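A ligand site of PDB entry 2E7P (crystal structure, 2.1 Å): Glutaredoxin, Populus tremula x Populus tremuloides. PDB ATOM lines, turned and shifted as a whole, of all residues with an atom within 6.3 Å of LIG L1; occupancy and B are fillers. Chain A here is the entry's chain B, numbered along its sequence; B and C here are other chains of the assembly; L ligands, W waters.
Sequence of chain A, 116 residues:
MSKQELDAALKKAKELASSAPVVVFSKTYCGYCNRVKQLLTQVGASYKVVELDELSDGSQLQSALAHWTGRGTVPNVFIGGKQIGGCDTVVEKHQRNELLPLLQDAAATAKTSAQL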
ATOM      1  N   LYS A  27     -12.076  25.419  12.764  1.00  0.00           N
ATOM      2  CA  LYS A  27     -13.195  26.390  12.517  1.00  0.00           C
ATOM      3  C   LYS A  27     -13.899  26.672  13.834  1.00  0.00           C
ATOM      4  O   LYS A  27     -14.066  25.769  14.680  1.00  0.00           O
ATOM      5  CB  LYS A  27     -14.182  25.872  11.474  1.00  0.00           C
ATOM      6  CG  LYS A  27     -13.601  25.843  10.055  1.00  0.00           C
ATOM      7  CD  LYS A  27     -14.567  25.234   9.044  1.00  0.00           C
ATOM      8  CE  LYS A  27     -13.987  25.309   7.649  1.00  0.00           C
ATOM      9  NZ  LYS A  27     -14.683  24.349   6.699  1.00  0.00           N
ATOM     10  N   TYR A  29     -16.768  27.080  14.904  1.00  0.00           N
ATOM     11  CA  TYR A  29     -18.061  26.477  15.314  1.00  0.00           C
ATOM     12  C   TYR A  29     -17.969  24.966  15.419  1.00  0.00           C
ATOM     13  O   TYR A  29     -18.941  24.274  15.837  1.00  0.00           O
ATOM     14  CB  TYR A  29     -19.171  26.843  14.296  1.00  0.00           C
ATOM     15  CG  TYR A  29     -18.842  26.392  12.896  1.00  0.00           C
ATOM     16  CD1 TYR A  29     -19.097  25.078  12.513  1.00  0.00           C
ATOM     17  CD2 TYR A  29     -18.248  27.251  11.973  1.00  0.00           C
ATOM     18  CE1 TYR A  29     -18.796  24.622  11.246  1.00  0.00           C
ATOM     19  CE2 TYR A  29     -17.938  26.803  10.670  1.00  0.00           C
ATOM     20  CZ  TYR A  29     -18.217  25.498  10.331  1.00  0.00           C
ATOM     21  OH  TYR A  29     -17.959  24.991   9.075  1.00  0.00           O
ATOM     22  N   CYS A  30     -16.817  24.417  15.003  1.00  0.00           N
ATOM     23  CA  CYS A  30     -16.663  22.961  14.890  1.00  0.00           C
ATOM     24  C   CYS A  30     -16.555  22.255  16.264  1.00  0.00           C
ATOM     25  O   CYS A  30     -15.619  22.503  17.002  1.00  0.00           O
ATOM     26  CB  CYS A  30     -15.471  22.627  13.973  1.00  0.00           C
ATOM     27  SG  CYS A  30     -15.096  20.879  13.903  1.00  0.00           S
ATOM     28  N   GLY A  31     -17.516  21.372  16.565  1.00  0.00           N
ATOM     29  CA  GLY A  31     -17.465  20.516  17.770  1.00  0.00           C
ATOM     30  C   GLY A  31     -16.208  19.653  17.982  1.00  0.00           C
ATOM     31  O   GLY A  31     -15.772  19.483  19.111  1.00  0.00           O
ATOM     32  N   TYR A  32     -15.649  19.106  16.904  1.00  0.00           N
ATOM     33  CA  TYR A  32     -14.364  18.388  16.954  1.00  0.00           C
ATOM     34  C   TYR A  32     -13.187  19.322  17.253  1.00  0.00           C
ATOM     35  O   TYR A  32     -12.238  18.946  17.965  1.00  0.00           O
ATOM     36  CB  TYR A  32     -14.123  17.632  15.646  1.00  0.00           C
ATOM     37  CG  TYR A  32     -14.941  16.368  15.501  1.00  0.00           C
ATOM     38  CD1 TYR A  32     -14.670  15.256  16.294  1.00  0.00           C
ATOM     39  CD2 TYR A  32     -15.985  16.272  14.560  1.00  0.00           C
ATOM     40  CE1 TYR A  32     -15.402  14.081  16.150  1.00  0.00           C
ATOM     41  CE2 TYR A  32     -16.728  15.093  14.430  1.00  0.00           C
ATOM     42  CZ  TYR A  32     -16.422  14.001  15.211  1.00  0.00           C
ATOM     43  OH  TYR A  32     -17.117  12.790  15.113  1.00  0.00           O
ATOM     44  N   CYS A  33     -13.226  20.534  16.727  1.00  0.00           N
ATOM     45  CA  CYS A  33     -12.223  21.506  17.058  1.00  0.00           C
ATOM     46  C   CYS A  33     -12.314  21.914  18.553  1.00  0.00           C
ATOM     47  O   CYS A  33     -11.284  22.021  19.251  1.00  0.00           O
ATOM     48  CB  CYS A  33     -12.310  22.742  16.143  1.00  0.00           C
ATOM     49  SG  CYS A  33     -11.905  22.351  14.447  1.00  0.00           S
ATOM     50  N   GLN A  62      -7.584  25.406   3.512  1.00  0.00           N
ATOM     51  CA  GLN A  62      -8.170  24.091   3.698  1.00  0.00           C
ATOM     52  C   GLN A  62      -7.893  23.183   2.510  1.00  0.00           C
ATOM     53  O   GLN A  62      -7.592  22.013   2.681  1.00  0.00           O
ATOM     54  CB  GLN A  62      -9.700  24.186   3.912  1.00  0.00           C
ATOM     55  CG  GLN A  62     -10.380  22.851   4.237  1.00  0.00           C
ATOM     56  CD  GLN A  62     -11.795  23.035   4.805  1.00  0.00           C
ATOM     57  OE1 GLN A  62     -12.283  24.159   4.925  1.00  0.00           O
ATOM     58  NE2 GLN A  62     -12.447  21.925   5.145  1.00  0.00           N
ATOM     59  N   ARG A  71      -6.233  15.027   4.283  1.00  0.00           N
ATOM     60  CA  ARG A  71      -7.293  15.244   5.262  1.00  0.00           C
ATOM     61  C   ARG A  71      -8.077  16.475   4.815  1.00  0.00           C
ATOM     62  O   ARG A  71      -7.506  17.561   4.645  1.00  0.00           O
ATOM     63  CB  ARG A  71      -6.725  15.460   6.679  1.00  0.00           C
ATOM     64  CG  ARG A  71      -7.766  15.779   7.784  1.00  0.00           C
ATOM     65  CD  ARG A  71      -7.120  15.780   9.185  1.00  0.00           C
ATOM     66  NE  ARG A  71      -6.780  14.400   9.534  1.00  0.00           N
ATOM     67  CZ  ARG A  71      -7.645  13.532  10.014  1.00  0.00           C
ATOM     68  NH1 ARG A  71      -8.898  13.914  10.275  1.00  0.00           N
ATOM     69  NH2 ARG A  71      -7.261  12.284  10.265  1.00  0.00           N
ATOM     70  N   GLY A  72      -9.385  16.272   4.629  1.00  0.00           N
ATOM     71  CA  GLY A  72     -10.273  17.325   4.126  1.00  0.00           C
ATOM     72  C   GLY A  72     -11.126  18.040   5.157  1.00  0.00           C
ATOM     73  O   GLY A  72     -11.910  18.940   4.815  1.00  0.00           O
ATOM     74  N   THR A  73     -10.950  17.684   6.430  1.00  0.00           N
ATOM     75  CA  THR A  73     -11.744  18.194   7.530  1.00  0.00           C
ATOM     76  C   THR A  73     -10.879  18.923   8.578  1.00  0.00           C
ATOM     77  O   THR A  73      -9.647  18.771   8.615  1.00  0.00           O
ATOM     78  CB  THR A  73     -12.494  17.028   8.231  1.00  0.00           C
ATOM     79  OG1 THR A  73     -11.548  16.053   8.713  1.00  0.00           O
ATOM     80  CG2 THR A  73     -13.512  16.340   7.305  1.00  0.00           C
ATOM     81  N   VAL A  74     -11.541  19.745   9.407  1.00  0.00           N
ATOM     82  CA  VAL A  74     -10.972  20.343  10.610  1.00  0.00           C
ATOM     83  C   VAL A  74     -11.466  19.533  11.850  1.00  0.00           C
ATOM     84  O   VAL A  74     -12.597  19.008  11.849  1.00  0.00           O
ATOM     85  CB  VAL A  74     -11.343  21.838  10.730  1.00  0.00           C
ATOM     86  CG1 VAL A  74     -10.657  22.692   9.622  1.00  0.00           C
ATOM     87  CG2 VAL A  74     -12.898  22.028  10.690  1.00  0.00           C
ATOM     88  N   PRO A  75     -10.641  19.413  12.903  1.00  0.00           N
ATOM     89  CA  PRO A  75      -9.319  20.028  13.012  1.00  0.00           C
ATOM     90  C   PRO A  75      -8.219  19.268  12.242  1.00  0.00           C
ATOM     91  O   PRO A  75      -8.377  18.108  11.904  1.00  0.00           O
ATOM     92  CB  PRO A  75      -9.039  20.013  14.516  1.00  0.00           C
ATOM     93  CG  PRO A  75      -9.733  18.749  15.014  1.00  0.00           C
ATOM     94  CD  PRO A  75     -10.982  18.610  14.102  1.00  0.00           C
ATOM     95  N   GLY A  85      -3.125  14.453  12.739  1.00  0.00           N
ATOM     96  CA  GLY A  85      -4.410  14.096  12.191  1.00  0.00           C
ATOM     97  C   GLY A  85      -5.499  14.966  12.811  1.00  0.00           C
ATOM     98  O   GLY A  85      -5.256  16.147  13.107  1.00  0.00           O
ATOM     99  N   GLY A  86      -6.671  14.368  12.986  1.00  0.00           N
ATOM    100  CA  GLY A  86      -7.857  15.124  13.456  1.00  0.00           C
ATOM    101  C   GLY A  86      -8.154  14.939  14.935  1.00  0.00           C
ATOM    102  O   GLY A  86      -7.293  14.510  15.721  1.00  0.00           O
ATOM    103  N   CYS A  87      -9.390  15.246  15.341  1.00  0.00           N
ATOM    104  CA  CYS A  87      -9.752  15.131  16.729  1.00  0.00           C
ATOM    105  C   CYS A  87      -9.713  13.668  17.178  1.00  0.00           C
ATOM    106  O   CYS A  87      -9.142  13.355  18.259  1.00  0.00           O
ATOM    107  CB  CYS A  87     -11.106  15.800  17.011  1.00  0.00           C
ATOM    108  SG  CYS A  87     -11.674  15.671  18.715  1.00  0.00           S
ATOM    109  N   ASP A  88     -10.272  12.768  16.376  1.00  0.00           N
ATOM    110  CA  ASP A  88     -10.247  11.333  16.736  1.00  0.00           C
ATOM    111  C   ASP A  88      -8.813  10.826  16.973  1.00  0.00           C
ATOM    112  O   ASP A  88      -8.560  10.036  17.889  1.00  0.00           O
ATOM    113  CB  ASP A  88     -10.923  10.447  15.697  1.00  0.00           C
ATOM    114  CG  ASP A  88     -12.442  10.610  15.668  1.00  0.00           C
ATOM    115  OD1 ASP A  88     -13.056  11.167  16.605  1.00  0.00           O
ATOM    116  OD2 ASP A  88     -12.995  10.149  14.666  1.00  0.00           O
ATOM    117  N   THR A  89      -7.894  11.267  16.108  1.00  0.00           N
ATOM    118  CA  THR A  89      -6.507  10.777  16.169  1.00  0.00           C
ATOM    119  C   THR A  89      -5.855  11.262  17.442  1.00  0.00           C
ATOM    120  O   THR A  89      -5.224  10.495  18.155  1.00  0.00           O
ATOM    121  CB  THR A  89      -5.669  11.283  14.984  1.00  0.00           C
ATOM    122  OG1 THR A  89      -6.397  11.033  13.786  1.00  0.00           O
ATOM    123  CG2 THR A  89      -4.301  10.532  14.923  1.00  0.00           C
ATOM    124  N   THR B  28     -22.719  13.760  14.797  1.00  0.00           N
ATOM    125  CA  THR B  28     -21.365  14.313  14.675  1.00  0.00           C
ATOM    126  C   THR B  28     -20.924  14.366  13.216  1.00  0.00           C
ATOM    127  O   THR B  28     -20.129  15.205  12.832  1.00  0.00           O
ATOM    128  CB  THR B  28     -20.337  13.453  15.436  1.00  0.00           C
ATOM    129  OG1 THR B  28     -20.428  12.095  14.961  1.00  0.00           O
ATOM    130  CG2 THR B  28     -20.599  13.503  16.969  1.00  0.00           C
ATOM    131  N   TYR B  29     -21.464  13.462  12.411  1.00  0.00           N
ATOM    132  CA  TYR B  29     -21.080  13.385  11.011  1.00  0.00           C
ATOM    133  C   TYR B  29     -21.835  14.341  10.067  1.00  0.00           C
ATOM    134  O   TYR B  29     -21.510  14.387   8.874  1.00  0.00           O
ATOM    135  CB  TYR B  29     -21.227  11.930  10.532  1.00  0.00           C
ATOM    136  CG  TYR B  29     -22.618  11.369  10.706  1.00  0.00           C
ATOM    137  CD1 TYR B  29     -23.653  11.730   9.823  1.00  0.00           C
ATOM    138  CD2 TYR B  29     -22.909  10.499  11.766  1.00  0.00           C
ATOM    139  CE1 TYR B  29     -24.926  11.233   9.978  1.00  0.00           C
ATOM    140  CE2 TYR B  29     -24.196   9.979  11.940  1.00  0.00           C
ATOM    141  CZ  TYR B  29     -25.196  10.360  11.046  1.00  0.00           C
ATOM    142  OH  TYR B  29     -26.444   9.867  11.227  1.00  0.00           O
ATOM    143  N   ASN B  34     -23.597  20.884  11.431  1.00  0.00           N
ATOM    144  CA  ASN B  34     -22.518  21.922  11.454  1.00  0.00           C
ATOM    145  C   ASN B  34     -22.901  23.317  10.961  1.00  0.00           C
ATOM    146  O   ASN B  34     -22.404  24.306  11.465  1.00  0.00           O
ATOM    147  CB  ASN B  34     -21.299  21.425  10.683  1.00  0.00           C
ATOM    148  CG  ASN B  34     -20.700  20.158  11.322  1.00  0.00           C
ATOM    149  OD1 ASN B  34     -20.903  19.936  12.521  1.00  0.00           O
ATOM    150  ND2 ASN B  34     -20.036  19.328  10.537  1.00  0.00           N
ATOM    151  N   LYS B  37     -24.711  24.990  13.767  1.00  0.00           N
ATOM    152  CA  LYS B  37     -23.698  25.402  14.730  1.00  0.00           C
ATOM    153  C   LYS B  37     -22.997  26.677  14.270  1.00  0.00           C
ATOM    154  O   LYS B  37     -22.728  27.570  15.086  1.00  0.00           O
ATOM    155  CB  LYS B  37     -22.685  24.250  14.911  1.00  0.00           C
ATOM    156  CG  LYS B  37     -23.256  23.083  15.728  1.00  0.00           C
ATOM    157  CD  LYS B  37     -22.423  21.858  15.498  1.00  0.00           C
ATOM    158  CE  LYS B  37     -23.108  20.600  16.055  1.00  0.00           C
ATOM    159  NZ  LYS B  37     -22.165  19.465  16.044  1.00  0.00           N
ATOM    160  N   THR C  73     -14.248  16.082   1.339  1.00  0.00           N
ATOM    161  CA  THR C  73     -15.655  15.959   1.761  1.00  0.00           C
ATOM    162  C   THR C  73     -16.588  15.529   0.630  1.00  0.00           C
ATOM    163  O   THR C  73     -16.191  15.525  -0.540  1.00  0.00           O
ATOM    164  CB  THR C  73     -16.189  17.265   2.344  1.00  0.00           C
ATOM    165  OG1 THR C  73     -16.110  18.290   1.353  1.00  0.00           O
ATOM    166  CG2 THR C  73     -15.406  17.650   3.632  1.00  0.00           C
HETATM  167  N1  LIG L   1     -13.178  12.461  12.197  1.00  0.00           N
HETATM  168  C1  LIG L   1     -12.754  13.844  11.980  1.00  0.00           C
HETATM  169  C2  LIG L   1     -11.936  14.244  13.172  1.00  0.00           C
HETATM  170  O1  LIG L   1     -11.310  15.326  13.224  1.00  0.00           O
HETATM  171  O2  LIG L   1     -11.938  13.450  14.136  1.00  0.00           O
HETATM  172  C3  LIG L   1     -14.041  14.693  11.903  1.00  0.00           C
HETATM  173  C4  LIG L   1     -13.874  16.214  11.673  1.00  0.00           C
HETATM  174  C5  LIG L   1     -15.126  16.862  11.067  1.00  0.00           C
HETATM  175  O3  LIG L   1     -16.126  16.186  10.821  1.00  0.00           O
HETATM  176  N2  LIG L   1     -15.104  18.179  10.837  1.00  0.00           N
HETATM  177  C6  LIG L   1     -16.186  18.904  10.188  1.00  0.00           C
HETATM  178  C7  LIG L   1     -15.646  19.329   8.848  1.00  0.00           C
HETATM  179  O4  LIG L   1     -14.466  19.597   8.755  1.00  0.00           O
HETATM  180  C8  LIG L   1     -16.425  20.190  10.944  1.00  0.00           C
HETATM  181  S1  LIG L   1     -17.235  19.868  12.516  1.00  0.00           S
HETATM  182  N3  LIG L   1     -16.457  19.464   7.788  1.00  0.00           N
HETATM  183  C9  LIG L   1     -16.035  19.909   6.465  1.00  0.00           C
HETATM  184  C10 LIG L   1     -15.707  21.392   6.459  1.00  0.00           C
HETATM  185  O5  LIG L   1     -15.907  22.110   7.475  1.00  0.00           O
HETATM  186  O6  LIG L   1     -15.242  21.914   5.433  1.00  0.00           O
HETATM  187  N1  LG2 L   2     -19.133  23.058   2.018  1.00  0.00           N
HETATM  188  C1  LG2 L   2     -19.309  21.661   1.697  1.00  0.00           C
HETATM  189  C2  LG2 L   2     -20.176  21.572   0.468  1.00  0.00           C
HETATM  190  O1  LG2 L   2     -20.270  20.514  -0.176  1.00  0.00           O
HETATM  191  O2  LG2 L   2     -20.717  22.611   0.125  1.00  0.00           O
HETATM  192  C3  LG2 L   2     -19.927  20.887   2.864  1.00  0.00           C
HETATM  193  C4  LG2 L   2     -19.568  19.425   2.738  1.00  0.00           C
HETATM  194  C5  LG2 L   2     -19.609  18.660   4.028  1.00  0.00           C
HETATM  195  O3  LG2 L   2     -19.556  19.245   5.109  1.00  0.00           O
HETATM  196  N2  LG2 L   2     -19.675  17.330   3.890  1.00  0.00           N
HETATM  197  C6  LG2 L   2     -19.727  16.430   5.020  1.00  0.00           C
HETATM  198  C7  LG2 L   2     -18.495  15.531   5.005  1.00  0.00           C
HETATM  199  O4  LG2 L   2     -18.024  15.117   3.947  1.00  0.00           O
HETATM  200  C8  LG2 L   2     -21.083  15.633   5.022  1.00  0.00           C
HETATM  201  S1  LG2 L   2     -22.785  16.315   5.143  1.00  0.00           S
HETATM  202  N3  LG2 L   2     -17.906  15.209   6.169  1.00  0.00           N
HETATM  203  C9  LG2 L   2     -16.702  14.378   6.309  1.00  0.00           C
HETATM  204  C10 LG2 L   2     -16.851  12.929   5.881  1.00  0.00           C
HETATM  205  O5  LG2 L   2     -18.002  12.455   5.690  1.00  0.00           O
HETATM  206  O6  LG2 L   2     -15.822  12.215   5.767  1.00  0.00           O
HETATM  207  O   HOH W   1     -19.416  19.898  14.938  1.00  0.00           O
HETATM  208  O   HOH W   2     -18.227  22.473   8.646  1.00  0.00           O
HETATM  209  O   HOH W   3     -18.799  16.499  10.899  1.00  0.00           O
HETATM  210  O   HOH W   4     -15.205  11.076  13.672  1.00  0.00           O
HETATM  211  O   HOH W   5      -8.889  11.956  13.352  1.00  0.00           O
HETATM  212  O   HOH W   6     -10.341  16.373  11.049  1.00  0.00           O
HETATM  213  O   HOH W   7     -19.351  18.667   7.969  1.00  0.00           O
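Residues that only touch LIG L1: Tyr 29 of chain A (3.9 Å), Tyr 32 (3.6 Å), Thr 73 of chain A (3.3 Å), Pro 75 (3.4 Å), Gly 86 (3.5 Å) and Thr 73 of chain C (3.7 Å). Hydrophobic or aromatic side chains that line LIG L1: Tyr 32, Val 74 and Pro 75. Of the 22 residues printed, 13 come within 4 Å of LIG L1.
Water W6 lies within hydrogen-bond range of an oxygen (O1) of LIG L1 (2.6 Å), the side-chain hydroxyl (OG1) of Thr 73 of chain A (2.6 Å), the backbone carbonyl oxygen (O) of Pro 75 (2.8 Å) and the guanidinium group (NH1) of Arg 71 (3.0 Å). Water W2 bridges the side-chain hydroxyl of Tyr 29 of chain A and an oxygen (O5) of LIG L1. Water W4 lies within hydrogen-bond range of OD2 of Asp 88 (2.6 Å), N1 of LIG L1 (2.9 Å) and OH of Tyr 32 (2.9 Å). Water W7 lies within hydrogen-bond range of the side-chain amide nitrogen (ND2) of Asn 34 of chain B (2.7 Å), an oxygen (O3) of LG2 L2 (2.9 Å) and a nitrogen (N3) of LIG L1 (3.0 Å). Water W1 lies within hydrogen-bond range of OD1 of Asn 34 of chain B (2.8 Å), N of Gly 31 (2.9 Å), NZ of Lys 37 of chain B (3.0 Å) and S1 of LIG L1 (3.3 Å). Water W5 lies within hydrogen-bond range of OG1 of Thr 89, N of Gly 86, N of Asp 88 and O2 of LIG L1.
N2 of LIG L1 is in hydrogen-bond range of O of Val 74 (2.8 Å). The backbone NH (N) of Val 74 is in hydrogen-bond range of an oxygen (O4) of LIG L1, at 3.0 Å. An oxygen (O5) of LIG L1 is in salt-bridge range of the side-chain amino group (NZ) of Lys 27 (2.7 Å). A nitrogen (N1) of LIG L1 lies within salt-bridge range of the side-chain carboxylate (OD2) of Asp 88, at 3.4 Å. The side-chain amide nitrogen of Asn 34 of chain B sits close to a sulfur (S1) of LIG L1 (3.5 Å). The side-chain amide nitrogen (NE2) of Gln 62 is in hydrogen-bond range of an oxygen (O6) of LIG L1 (2.8 Å). N of Cys 87 lies within hydrogen-bond range of O1 of LIG L1, 2.9 Å away. SG of Cys 30 lies close to S1 of LIG L1 (2.7 Å). The backbone NH (N) of Asp 88 sits at hydrogen-bond distance from an oxygen (O2) of LIG L1 (2.9 Å).
OG1 of Thr 89 is in hydrogen-bond range of N of Gly 86 (3.4 Å). The side-chain amino group of Lys 27 is in hydrogen-bond range of the side-chain amide oxygen of Gln 62 (3.0 Å). N of Lys 27 is in hydrogen-bond range of SG of Cys 33 (3.5 Å). The backbone NH (N) of Cys 33 sits at hydrogen-bond distance from the side-chain sulfur (SG) of Cys 30 (3.4 Å). The backbone NH (N) of Tyr 32 sits close to the side-chain sulfur (SG) of Cys 30 (3.5 Å). The side-chain hydroxyl (OH) of Tyr 32 sits close to the side-chain hydroxyl (OG1) of Thr 28 of chain B. The side-chain sulfur (SG) of Cys 30 lies within hydrogen-bond range of the backbone carbonyl oxygen (O) of Val 74, at 3.7 Å. O of Gly 72 lies within hydrogen-bond range of NE2 of Gln 62.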
